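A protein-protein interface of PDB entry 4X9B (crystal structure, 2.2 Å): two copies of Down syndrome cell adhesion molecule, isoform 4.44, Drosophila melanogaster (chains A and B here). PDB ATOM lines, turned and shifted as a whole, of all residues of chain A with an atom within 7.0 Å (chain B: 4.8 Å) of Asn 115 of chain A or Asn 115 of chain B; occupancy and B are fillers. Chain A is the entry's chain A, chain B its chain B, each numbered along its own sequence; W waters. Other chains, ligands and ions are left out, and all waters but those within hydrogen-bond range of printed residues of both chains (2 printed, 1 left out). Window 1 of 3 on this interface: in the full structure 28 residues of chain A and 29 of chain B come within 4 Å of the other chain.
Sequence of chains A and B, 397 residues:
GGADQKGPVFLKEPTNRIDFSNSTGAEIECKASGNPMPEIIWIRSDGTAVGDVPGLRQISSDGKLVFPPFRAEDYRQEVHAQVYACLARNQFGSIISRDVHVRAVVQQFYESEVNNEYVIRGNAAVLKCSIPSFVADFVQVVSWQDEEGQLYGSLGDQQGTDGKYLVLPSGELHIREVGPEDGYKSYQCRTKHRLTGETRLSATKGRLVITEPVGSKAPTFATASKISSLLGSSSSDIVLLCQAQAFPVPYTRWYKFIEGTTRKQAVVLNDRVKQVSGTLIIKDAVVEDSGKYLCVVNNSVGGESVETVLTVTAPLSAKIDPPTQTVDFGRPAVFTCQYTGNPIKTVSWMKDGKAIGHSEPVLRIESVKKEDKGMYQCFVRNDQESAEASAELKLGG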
ATOM      1  N   GLU A 113       5.373  -4.513  27.582  1.00  0.00           N
ATOM      2  CA  GLU A 113       6.382  -5.513  27.258  1.00  0.00           C
ATOM      3  C   GLU A 113       7.225  -5.123  26.034  1.00  0.00           C
ATOM      4  O   GLU A 113       6.749  -4.429  25.126  1.00  0.00           O
ATOM      5  CB  GLU A 113       5.714  -6.862  27.015  1.00  0.00           C
ATOM      6  CG  GLU A 113       5.089  -7.477  28.269  1.00  0.00           C
ATOM      7  CD  GLU A 113       4.726  -8.938  28.084  1.00  0.00           C
ATOM      8  OE1 GLU A 113       4.960  -9.480  26.980  1.00  0.00           O
ATOM      9  OE2 GLU A 113       4.206  -9.548  29.047  1.00  0.00           O
ATOM     10  N   VAL A 114       8.483  -5.561  26.034  1.00  0.00           N
ATOM     11  CA  VAL A 114       9.341  -5.467  24.857  1.00  0.00           C
ATOM     12  C   VAL A 114       9.630  -6.874  24.348  1.00  0.00           C
ATOM     13  O   VAL A 114      10.335  -7.641  24.993  1.00  0.00           O
ATOM     14  CB  VAL A 114      10.660  -4.749  25.159  1.00  0.00           C
ATOM     15  CG1 VAL A 114      11.468  -4.563  23.881  1.00  0.00           C
ATOM     16  CG2 VAL A 114      10.397  -3.403  25.807  1.00  0.00           C
ATOM     17  N   ASN A 115       9.057  -7.209  23.199  1.00  0.00           N
ATOM     18  CA  ASN A 115       9.298  -8.498  22.557  1.00  0.00           C
ATOM     19  C   ASN A 115      10.623  -8.511  21.798  1.00  0.00           C
ATOM     20  O   ASN A 115      11.132  -7.463  21.405  1.00  0.00           O
ATOM     21  CB  ASN A 115       8.156  -8.840  21.603  1.00  0.00           C
ATOM     22  CG  ASN A 115       6.816  -8.960  22.314  1.00  0.00           C
ATOM     23  OD1 ASN A 115       6.751  -9.143  23.537  1.00  0.00           O
ATOM     24  ND2 ASN A 115       5.738  -8.867  21.548  1.00  0.00           N
ATOM     25  N   ASN A 116      11.181  -9.700  21.605  1.00  0.00           N
ATOM     26  CA  ASN A 116      12.386  -9.836  20.820  1.00  0.00           C
ATOM     27  C   ASN A 116      12.093  -9.535  19.363  1.00  0.00           C
ATOM     28  O   ASN A 116      10.951  -9.639  18.907  1.00  0.00           O
ATOM     29  CB  ASN A 116      12.976 -11.234  20.946  1.00  0.00           C
ATOM     30  CG  ASN A 116      13.571 -11.502  22.311  1.00  0.00           C
ATOM     31  OD1 ASN A 116      13.928 -10.584  23.050  1.00  0.00           O
ATOM     32  ND2 ASN A 116      13.681 -12.775  22.651  1.00  0.00           N
ATOM     33  N   GLU A 117      13.137  -9.163  18.637  1.00  0.00           N
ATOM     34  CA  GLU A 117      13.012  -8.865  17.219  1.00  0.00           C
ATOM     35  C   GLU A 117      14.081  -9.636  16.460  1.00  0.00           C
ATOM     36  O   GLU A 117      15.248  -9.643  16.853  1.00  0.00           O
ATOM     37  CB  GLU A 117      13.136  -7.359  16.976  1.00  0.00           C
ATOM     38  CG  GLU A 117      12.211  -6.826  15.888  1.00  0.00           C
ATOM     39  CD  GLU A 117      10.733  -6.904  16.257  1.00  0.00           C
ATOM     40  OE1 GLU A 117      10.358  -6.502  17.380  1.00  0.00           O
ATOM     41  OE2 GLU A 117       9.942  -7.361  15.407  1.00  0.00           O
ATOM     42  N   VAL A 126      13.651  -2.438  14.617  1.00  0.00           N
ATOM     43  CA  VAL A 126      12.726  -1.610  15.385  1.00  0.00           C
ATOM     44  C   VAL A 126      12.171  -2.392  16.579  1.00  0.00           C
ATOM     45  O   VAL A 126      11.496  -3.402  16.402  1.00  0.00           O
ATOM     46  CB  VAL A 126      11.557  -1.117  14.509  1.00  0.00           C
ATOM     47  CG1 VAL A 126      10.571  -0.300  15.329  1.00  0.00           C
ATOM     48  CG2 VAL A 126      12.082  -0.288  13.354  1.00  0.00           C
ATOM     49  N   LEU A 127      12.469  -1.922  17.787  1.00  0.00           N
ATOM     50  CA  LEU A 127      11.933  -2.525  18.998  1.00  0.00           C
ATOM     51  C   LEU A 127      10.681  -1.772  19.408  1.00  0.00           C
ATOM     52  O   LEU A 127      10.689  -0.544  19.473  1.00  0.00           O
ATOM     53  CB  LEU A 127      12.968  -2.498  20.124  1.00  0.00           C
ATOM     54  CG  LEU A 127      14.075  -3.550  20.073  1.00  0.00           C
ATOM     55  CD1 LEU A 127      15.215  -3.151  20.985  1.00  0.00           C
ATOM     56  CD2 LEU A 127      13.541  -4.918  20.467  1.00  0.00           C
ATOM     57  N   LYS A 128       9.606  -2.508  19.676  1.00  0.00           N
ATOM     58  CA  LYS A 128       8.336  -1.894  20.049  1.00  0.00           C
ATOM     59  C   LYS A 128       8.035  -2.067  21.526  1.00  0.00           C
ATOM     60  O   LYS A 128       8.339  -3.103  22.134  1.00  0.00           O
ATOM     61  CB  LYS A 128       7.183  -2.481  19.233  1.00  0.00           C
ATOM     62  CG  LYS A 128       7.347  -2.335  17.732  1.00  0.00           C
ATOM     63  CD  LYS A 128       7.767  -3.662  17.122  1.00  0.00           C
ATOM     64  CE  LYS A 128       7.901  -3.587  15.612  1.00  0.00           C
ATOM     65  NZ  LYS A 128       8.266  -4.920  15.051  1.00  0.00           N
ATOM     66  N   CYS A 129       7.422  -1.037  22.092  1.00  0.00           N
ATOM     67  CA  CYS A 129       6.903  -1.108  23.436  1.00  0.00           C
ATOM     68  C   CYS A 129       5.445  -1.534  23.324  1.00  0.00           C
ATOM     69  O   CYS A 129       4.598  -0.750  22.897  1.00  0.00           O
ATOM     70  CB  CYS A 129       7.041   0.255  24.120  1.00  0.00           C
ATOM     71  SG  CYS A 129       6.532   0.316  25.849  1.00  0.00           S
ATOM     72  N   SER A 130       5.141  -2.760  23.736  1.00  0.00           N
ATOM     73  CA  SER A 130       3.787  -3.282  23.564  1.00  0.00           C
ATOM     74  C   SER A 130       2.970  -2.904  24.777  1.00  0.00           C
ATOM     75  O   SER A 130       3.226  -3.369  25.890  1.00  0.00           O
ATOM     76  CB  SER A 130       3.775  -4.807  23.393  1.00  0.00           C
ATOM     77  OG  SER A 130       4.187  -5.191  22.096  1.00  0.00           O
ATOM     78  N   TRP A 144      13.755   4.776  26.829  1.00  0.00           N
ATOM     79  CA  TRP A 144      14.156   3.383  26.746  1.00  0.00           C
ATOM     80  C   TRP A 144      15.361   3.179  27.641  1.00  0.00           C
ATOM     81  O   TRP A 144      16.083   4.129  27.941  1.00  0.00           O
ATOM     82  CB  TRP A 144      14.475   2.985  25.314  1.00  0.00           C
ATOM     83  CG  TRP A 144      13.263   2.723  24.496  1.00  0.00           C
ATOM     84  CD1 TRP A 144      12.441   3.652  23.916  1.00  0.00           C
ATOM     85  CD2 TRP A 144      12.728   1.445  24.157  1.00  0.00           C
ATOM     86  NE1 TRP A 144      11.429   3.024  23.239  1.00  0.00           N
ATOM     87  CE2 TRP A 144      11.584   1.669  23.367  1.00  0.00           C
ATOM     88  CE3 TRP A 144      13.106   0.132  24.440  1.00  0.00           C
ATOM     89  CZ2 TRP A 144      10.820   0.627  22.854  1.00  0.00           C
ATOM     90  CZ3 TRP A 144      12.341  -0.899  23.934  1.00  0.00           C
ATOM     91  CH2 TRP A 144      11.213  -0.646  23.151  1.00  0.00           C
ATOM     92  N   TYR A 187      16.731  -4.448  26.116  1.00  0.00           N
ATOM     93  CA  TYR A 187      16.154  -3.137  26.365  1.00  0.00           C
ATOM     94  C   TYR A 187      14.784  -3.235  27.003  1.00  0.00           C
ATOM     95  O   TYR A 187      14.017  -4.158  26.735  1.00  0.00           O
ATOM     96  CB  TYR A 187      16.029  -2.348  25.064  1.00  0.00           C
ATOM     97  CG  TYR A 187      17.303  -2.222  24.263  1.00  0.00           C
ATOM     98  CD1 TYR A 187      17.686  -3.216  23.372  1.00  0.00           C
ATOM     99  CD2 TYR A 187      18.109  -1.093  24.377  1.00  0.00           C
ATOM    100  CE1 TYR A 187      18.841  -3.095  22.622  1.00  0.00           C
ATOM    101  CE2 TYR A 187      19.270  -0.965  23.632  1.00  0.00           C
ATOM    102  CZ  TYR A 187      19.628  -1.968  22.756  1.00  0.00           C
ATOM    103  OH  TYR A 187      20.777  -1.848  22.011  1.00  0.00           O
ATOM    104  N   THR A 204       8.915  -7.146  30.677  1.00  0.00           N
ATOM    105  CA  THR A 204       9.822  -8.023  29.933  1.00  0.00           C
ATOM    106  C   THR A 204      10.866  -7.197  29.178  1.00  0.00           C
ATOM    107  O   THR A 204      10.643  -6.020  28.880  1.00  0.00           O
ATOM    108  CB  THR A 204       9.065  -8.910  28.925  1.00  0.00           C
ATOM    109  OG1 THR A 204       8.426  -8.083  27.945  1.00  0.00           O
ATOM    110  CG2 THR A 204       8.015  -9.764  29.625  1.00  0.00           C
ATOM    111  N   LYS A 205      11.997  -7.831  28.875  1.00  0.00           N
ATOM    112  CA  LYS A 205      13.107  -7.202  28.161  1.00  0.00           C
ATOM    113  C   LYS A 205      13.224  -7.812  26.773  1.00  0.00           C
ATOM    114  O   LYS A 205      13.142  -9.033  26.635  1.00  0.00           O
ATOM    115  CB  LYS A 205      14.417  -7.397  28.928  1.00  0.00           C
ATOM    116  CG  LYS A 205      14.310  -7.099  30.412  1.00  0.00           C
ATOM    117  CD  LYS A 205      15.608  -7.354  31.158  1.00  0.00           C
ATOM    118  CE  LYS A 205      15.436  -7.068  32.650  1.00  0.00           C
ATOM    119  NZ  LYS A 205      16.719  -7.116  33.401  1.00  0.00           N
ATOM    120  N   GLY A 206      13.351  -6.978  25.742  1.00  0.00           N
ATOM    121  CA  GLY A 206      13.578  -7.481  24.398  1.00  0.00           C
ATOM    122  C   GLY A 206      15.022  -7.406  23.955  1.00  0.00           C
ATOM    123  O   GLY A 206      15.774  -6.555  24.424  1.00  0.00           O
ATOM    124  N   ARG A 207      15.385  -8.231  22.981  1.00  0.00           N
ATOM    125  CA  ARG A 207      16.733  -8.191  22.417  1.00  0.00           C
ATOM    126  C   ARG A 207      16.666  -8.481  20.936  1.00  0.00           C
ATOM    127  O   ARG A 207      15.700  -9.082  20.466  1.00  0.00           O
ATOM    128  CB  ARG A 207      17.665  -9.197  23.111  1.00  0.00           C
ATOM    129  CG  ARG A 207      17.396 -10.665  22.786  1.00  0.00           C
ATOM    130  CD  ARG A 207      18.282 -11.594  23.622  1.00  0.00           C
ATOM    131  NE  ARG A 207      17.734 -12.952  23.718  1.00  0.00           N
ATOM    132  CZ  ARG A 207      18.108 -13.985  22.961  1.00  0.00           C
ATOM    133  NH1 ARG A 207      19.048 -13.849  22.028  1.00  0.00           N
ATOM    134  NH2 ARG A 207      17.536 -15.169  23.141  1.00  0.00           N
ATOM    135  N   LEU A 208      17.696  -8.057  20.211  1.00  0.00           N
ATOM    136  CA  LEU A 208      17.821  -8.371  18.797  1.00  0.00           C
ATOM    137  C   LEU A 208      18.433  -9.749  18.616  1.00  0.00           C
ATOM    138  O   LEU A 208      19.533 -10.017  19.099  1.00  0.00           O
ATOM    139  CB  LEU A 208      18.679  -7.327  18.079  1.00  0.00           C
ATOM    140  CG  LEU A 208      18.275  -5.861  18.266  1.00  0.00           C
ATOM    141  CD1 LEU A 208      19.156  -4.964  17.402  1.00  0.00           C
ATOM    142  CD2 LEU A 208      16.805  -5.639  17.941  1.00  0.00           C
ATOM    143  N   GLU B 113       8.833 -17.894  18.821  1.00  0.00           N
ATOM    144  CA  GLU B 113       8.504 -17.458  20.168  1.00  0.00           C
ATOM    145  C   GLU B 113       7.001 -17.293  20.308  1.00  0.00           C
ATOM    146  O   GLU B 113       6.312 -17.008  19.334  1.00  0.00           O
ATOM    147  CB  GLU B 113       9.197 -16.134  20.499  1.00  0.00           C
ATOM    148  CG  GLU B 113      10.678 -16.252  20.773  1.00  0.00           C
ATOM    149  CD  GLU B 113      11.300 -14.923  21.167  1.00  0.00           C
ATOM    150  OE1 GLU B 113      10.554 -14.001  21.567  1.00  0.00           O
ATOM    151  OE2 GLU B 113      12.536 -14.797  21.072  1.00  0.00           O
ATOM    152  N   VAL B 114       6.498 -17.498  21.520  1.00  0.00           N
ATOM    153  CA  VAL B 114       5.135 -17.114  21.851  1.00  0.00           C
ATOM    154  C   VAL B 114       5.211 -16.011  22.893  1.00  0.00           C
ATOM    155  O   VAL B 114       5.600 -16.251  24.038  1.00  0.00           O
ATOM    156  CB  VAL B 114       4.307 -18.293  22.393  1.00  0.00           C
ATOM    157  CG1 VAL B 114       2.843 -17.895  22.512  1.00  0.00           C
ATOM    158  CG2 VAL B 114       4.448 -19.509  21.499  1.00  0.00           C
ATOM    159  N   ASN B 115       4.864 -14.798  22.483  1.00  0.00           N
ATOM    160  CA  ASN B 115       4.772 -13.668  23.396  1.00  0.00           C
ATOM    161  C   ASN B 115       3.457 -13.650  24.165  1.00  0.00           C
ATOM    162  O   ASN B 115       2.465 -14.232  23.734  1.00  0.00           O
ATOM    163  CB  ASN B 115       4.950 -12.366  22.634  1.00  0.00           C
ATOM    164  CG  ASN B 115       6.354 -12.213  22.081  1.00  0.00           C
ATOM    165  OD1 ASN B 115       7.341 -12.358  22.803  1.00  0.00           O
ATOM    166  ND2 ASN B 115       6.449 -11.948  20.789  1.00  0.00           N
ATOM    167  N   ASN B 116       3.462 -12.994  25.317  1.00  0.00           N
ATOM    168  CA  ASN B 116       2.263 -12.889  26.135  1.00  0.00           C
ATOM    169  C   ASN B 116       1.165 -12.085  25.453  1.00  0.00           C
ATOM    170  O   ASN B 116       1.436 -11.232  24.608  1.00  0.00           O
ATOM    171  CB  ASN B 116       2.599 -12.250  27.478  1.00  0.00           C
ATOM    172  CG  ASN B 116       3.586 -13.078  28.287  1.00  0.00           C
ATOM    173  OD1 ASN B 116       3.606 -14.305  28.203  1.00  0.00           O
ATOM    174  ND2 ASN B 116       4.412 -12.405  29.072  1.00  0.00           N
ATOM    175  N   GLU B 117      -0.075 -12.380  25.823  1.00  0.00           N
ATOM    176  CA  GLU B 117      -1.226 -11.617  25.369  1.00  0.00           C
ATOM    177  C   GLU B 117      -1.927 -11.022  26.576  1.00  0.00           C
ATOM    178  O   GLU B 117      -2.000 -11.641  27.637  1.00  0.00           O
ATOM    179  CB  GLU B 117      -2.179 -12.497  24.561  1.00  0.00           C
ATOM    180  CG  GLU B 117      -1.572 -13.030  23.283  1.00  0.00           C
ATOM    181  CD  GLU B 117      -1.233 -11.927  22.295  1.00  0.00           C
ATOM    182  OE1 GLU B 117      -1.773 -10.810  22.451  1.00  0.00           O
ATOM    183  OE2 GLU B 117      -0.425 -12.174  21.365  1.00  0.00           O
ATOM    184  N   LEU B 127      -3.519 -16.234  20.597  1.00  0.00           N
ATOM    185  CA  LEU B 127      -2.094 -16.425  20.788  1.00  0.00           C
ATOM    186  C   LEU B 127      -1.466 -16.555  19.420  1.00  0.00           C
ATOM    187  O   LEU B 127      -2.063 -17.138  18.513  1.00  0.00           O
ATOM    188  CB  LEU B 127      -1.801 -17.662  21.640  1.00  0.00           C
ATOM    189  CG  LEU B 127      -2.002 -17.573  23.159  1.00  0.00           C
ATOM    190  CD1 LEU B 127      -0.968 -16.666  23.808  1.00  0.00           C
ATOM    191  CD2 LEU B 127      -3.404 -17.101  23.490  1.00  0.00           C
ATOM    192  N   LYS B 128      -0.269 -16.001  19.275  1.00  0.00           N
ATOM    193  CA  LYS B 128       0.441 -16.026  18.008  1.00  0.00           C
ATOM    194  C   LYS B 128       1.795 -16.696  18.162  1.00  0.00           C
ATOM    195  O   LYS B 128       2.506 -16.483  19.146  1.00  0.00           O
ATOM    196  CB  LYS B 128       0.622 -14.607  17.465  1.00  0.00           C
ATOM    197  CG  LYS B 128      -0.599 -14.050  16.736  1.00  0.00           C
ATOM    198  CD  LYS B 128      -1.634 -13.448  17.680  1.00  0.00           C
ATOM    199  CE  LYS B 128      -1.195 -12.088  18.214  1.00  0.00           C
ATOM    200  NZ  LYS B 128      -2.293 -11.381  18.935  1.00  0.00           N
ATOM    201  N   SER B 130       5.275 -16.470  16.885  1.00  0.00           N
ATOM    202  CA  SER B 130       6.088 -15.456  16.232  1.00  0.00           C
ATOM    203  C   SER B 130       7.268 -16.108  15.539  1.00  0.00           C
ATOM    204  O   SER B 130       8.093 -16.754  16.188  1.00  0.00           O
ATOM    205  CB  SER B 130       6.573 -14.415  17.242  1.00  0.00           C
ATOM    206  OG  SER B 130       5.497 -13.611  17.697  1.00  0.00           O
ATOM    207  N   GLY B 206       4.183 -18.616  25.910  1.00  0.00           N
ATOM    208  CA  GLY B 206       3.427 -17.414  26.180  1.00  0.00           C
ATOM    209  C   GLY B 206       2.454 -17.640  27.322  1.00  0.00           C
ATOM    210  O   GLY B 206       2.084 -18.773  27.613  1.00  0.00           O
HETATM  211  O   HOH W   1       9.366 -11.761  19.624  1.00  0.00           O
HETATM  212  O   HOH W   2       5.996 -11.740  26.102  1.00  0.00           O
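The side-chain carboxylate (OE2) of Glu 113 of chain A is in hydrogen-bond range of the side-chain amide nitrogen (ND2) of Asn 116 of chain B (2.9 Å). ND2 of Asn 115 of chain B sits close to ND2 of Asn 115 of chain A. The side-chain carboxylate of Glu 113 of chain B sits at hydrogen-bond distance from the side-chain amide nitrogen of Asn 116 of chain A (2.8 Å).
Glu 113 of chain A touches Asn 116 of chain B, and with the chains exchanged Asn 116 of chain A touches Glu 113 of chain B. Asn 115 of chain B touches its own counterpart, Asn 115 of chain A. Of the 3 pairs that touch across the chains among the printed residues, 3 have their exchanged pair printed and touching as well.
Of chain B, only Asn 115 (3.3 Å) comes within 4 Å of Asn 115 of chain A. Of chain A, only Asn 115 (3.3 Å) comes within 4 Å of Asn 115 of chain B. Of the printed residues of chain B, Glu 113 of chain A touches Asn 116. Printed residues of chain B within 4 Å of Asn 116 of chain A: Glu 113. Of the printed residues of chain A, Asn 116 of chain B touches Glu 113 (2.9 Å). Gly 206 of chain B touches none of the printed residues of chain A. Trp 144 of chain A touches none of the printed residues of chain B. The nearest printed residue of chain B that does not touch Asn 115 of chain A is Asn 116 of chain B (5.4 Å).
Water W2 lies within hydrogen-bond range of OE1 of Glu 113 of chain A and N of Asn 116 of chain B. Water W1 lies within hydrogen-bond range of the backbone carbonyl oxygen (O) of Asn 116 of chain A (2.7 Å), the side-chain amide nitrogen (ND2) of Asn 115 of chain B (3.1 Å) and the side-chain carboxylate (OE1) of Glu 113 of chain B (3.2 Å).
The backbone carbonyl oxygen of Glu 113 of chain A sits at hydrogen-bond distance from the backbone NH of Ser 130 of chain A. OD1 of Asn 116 of chain A is in hydrogen-bond range of N of Arg 207 of chain A. N of Ser 130 of chain B is in hydrogen-bond range of O of Glu 113 of chain B, at 2.7 Å.
Along chain B the printed residues that touch a printed residue of chain A span positions 113 to 116. Of the 17 printed residues of chain A, 3 touch a printed residue of chain B. Among the printed residues, 3 pairs touch across the chains. Among the printed residues, no Asp or Glu carboxylate lies within 4 Å of a Lys or Arg side-chain nitrogen of the other chain.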
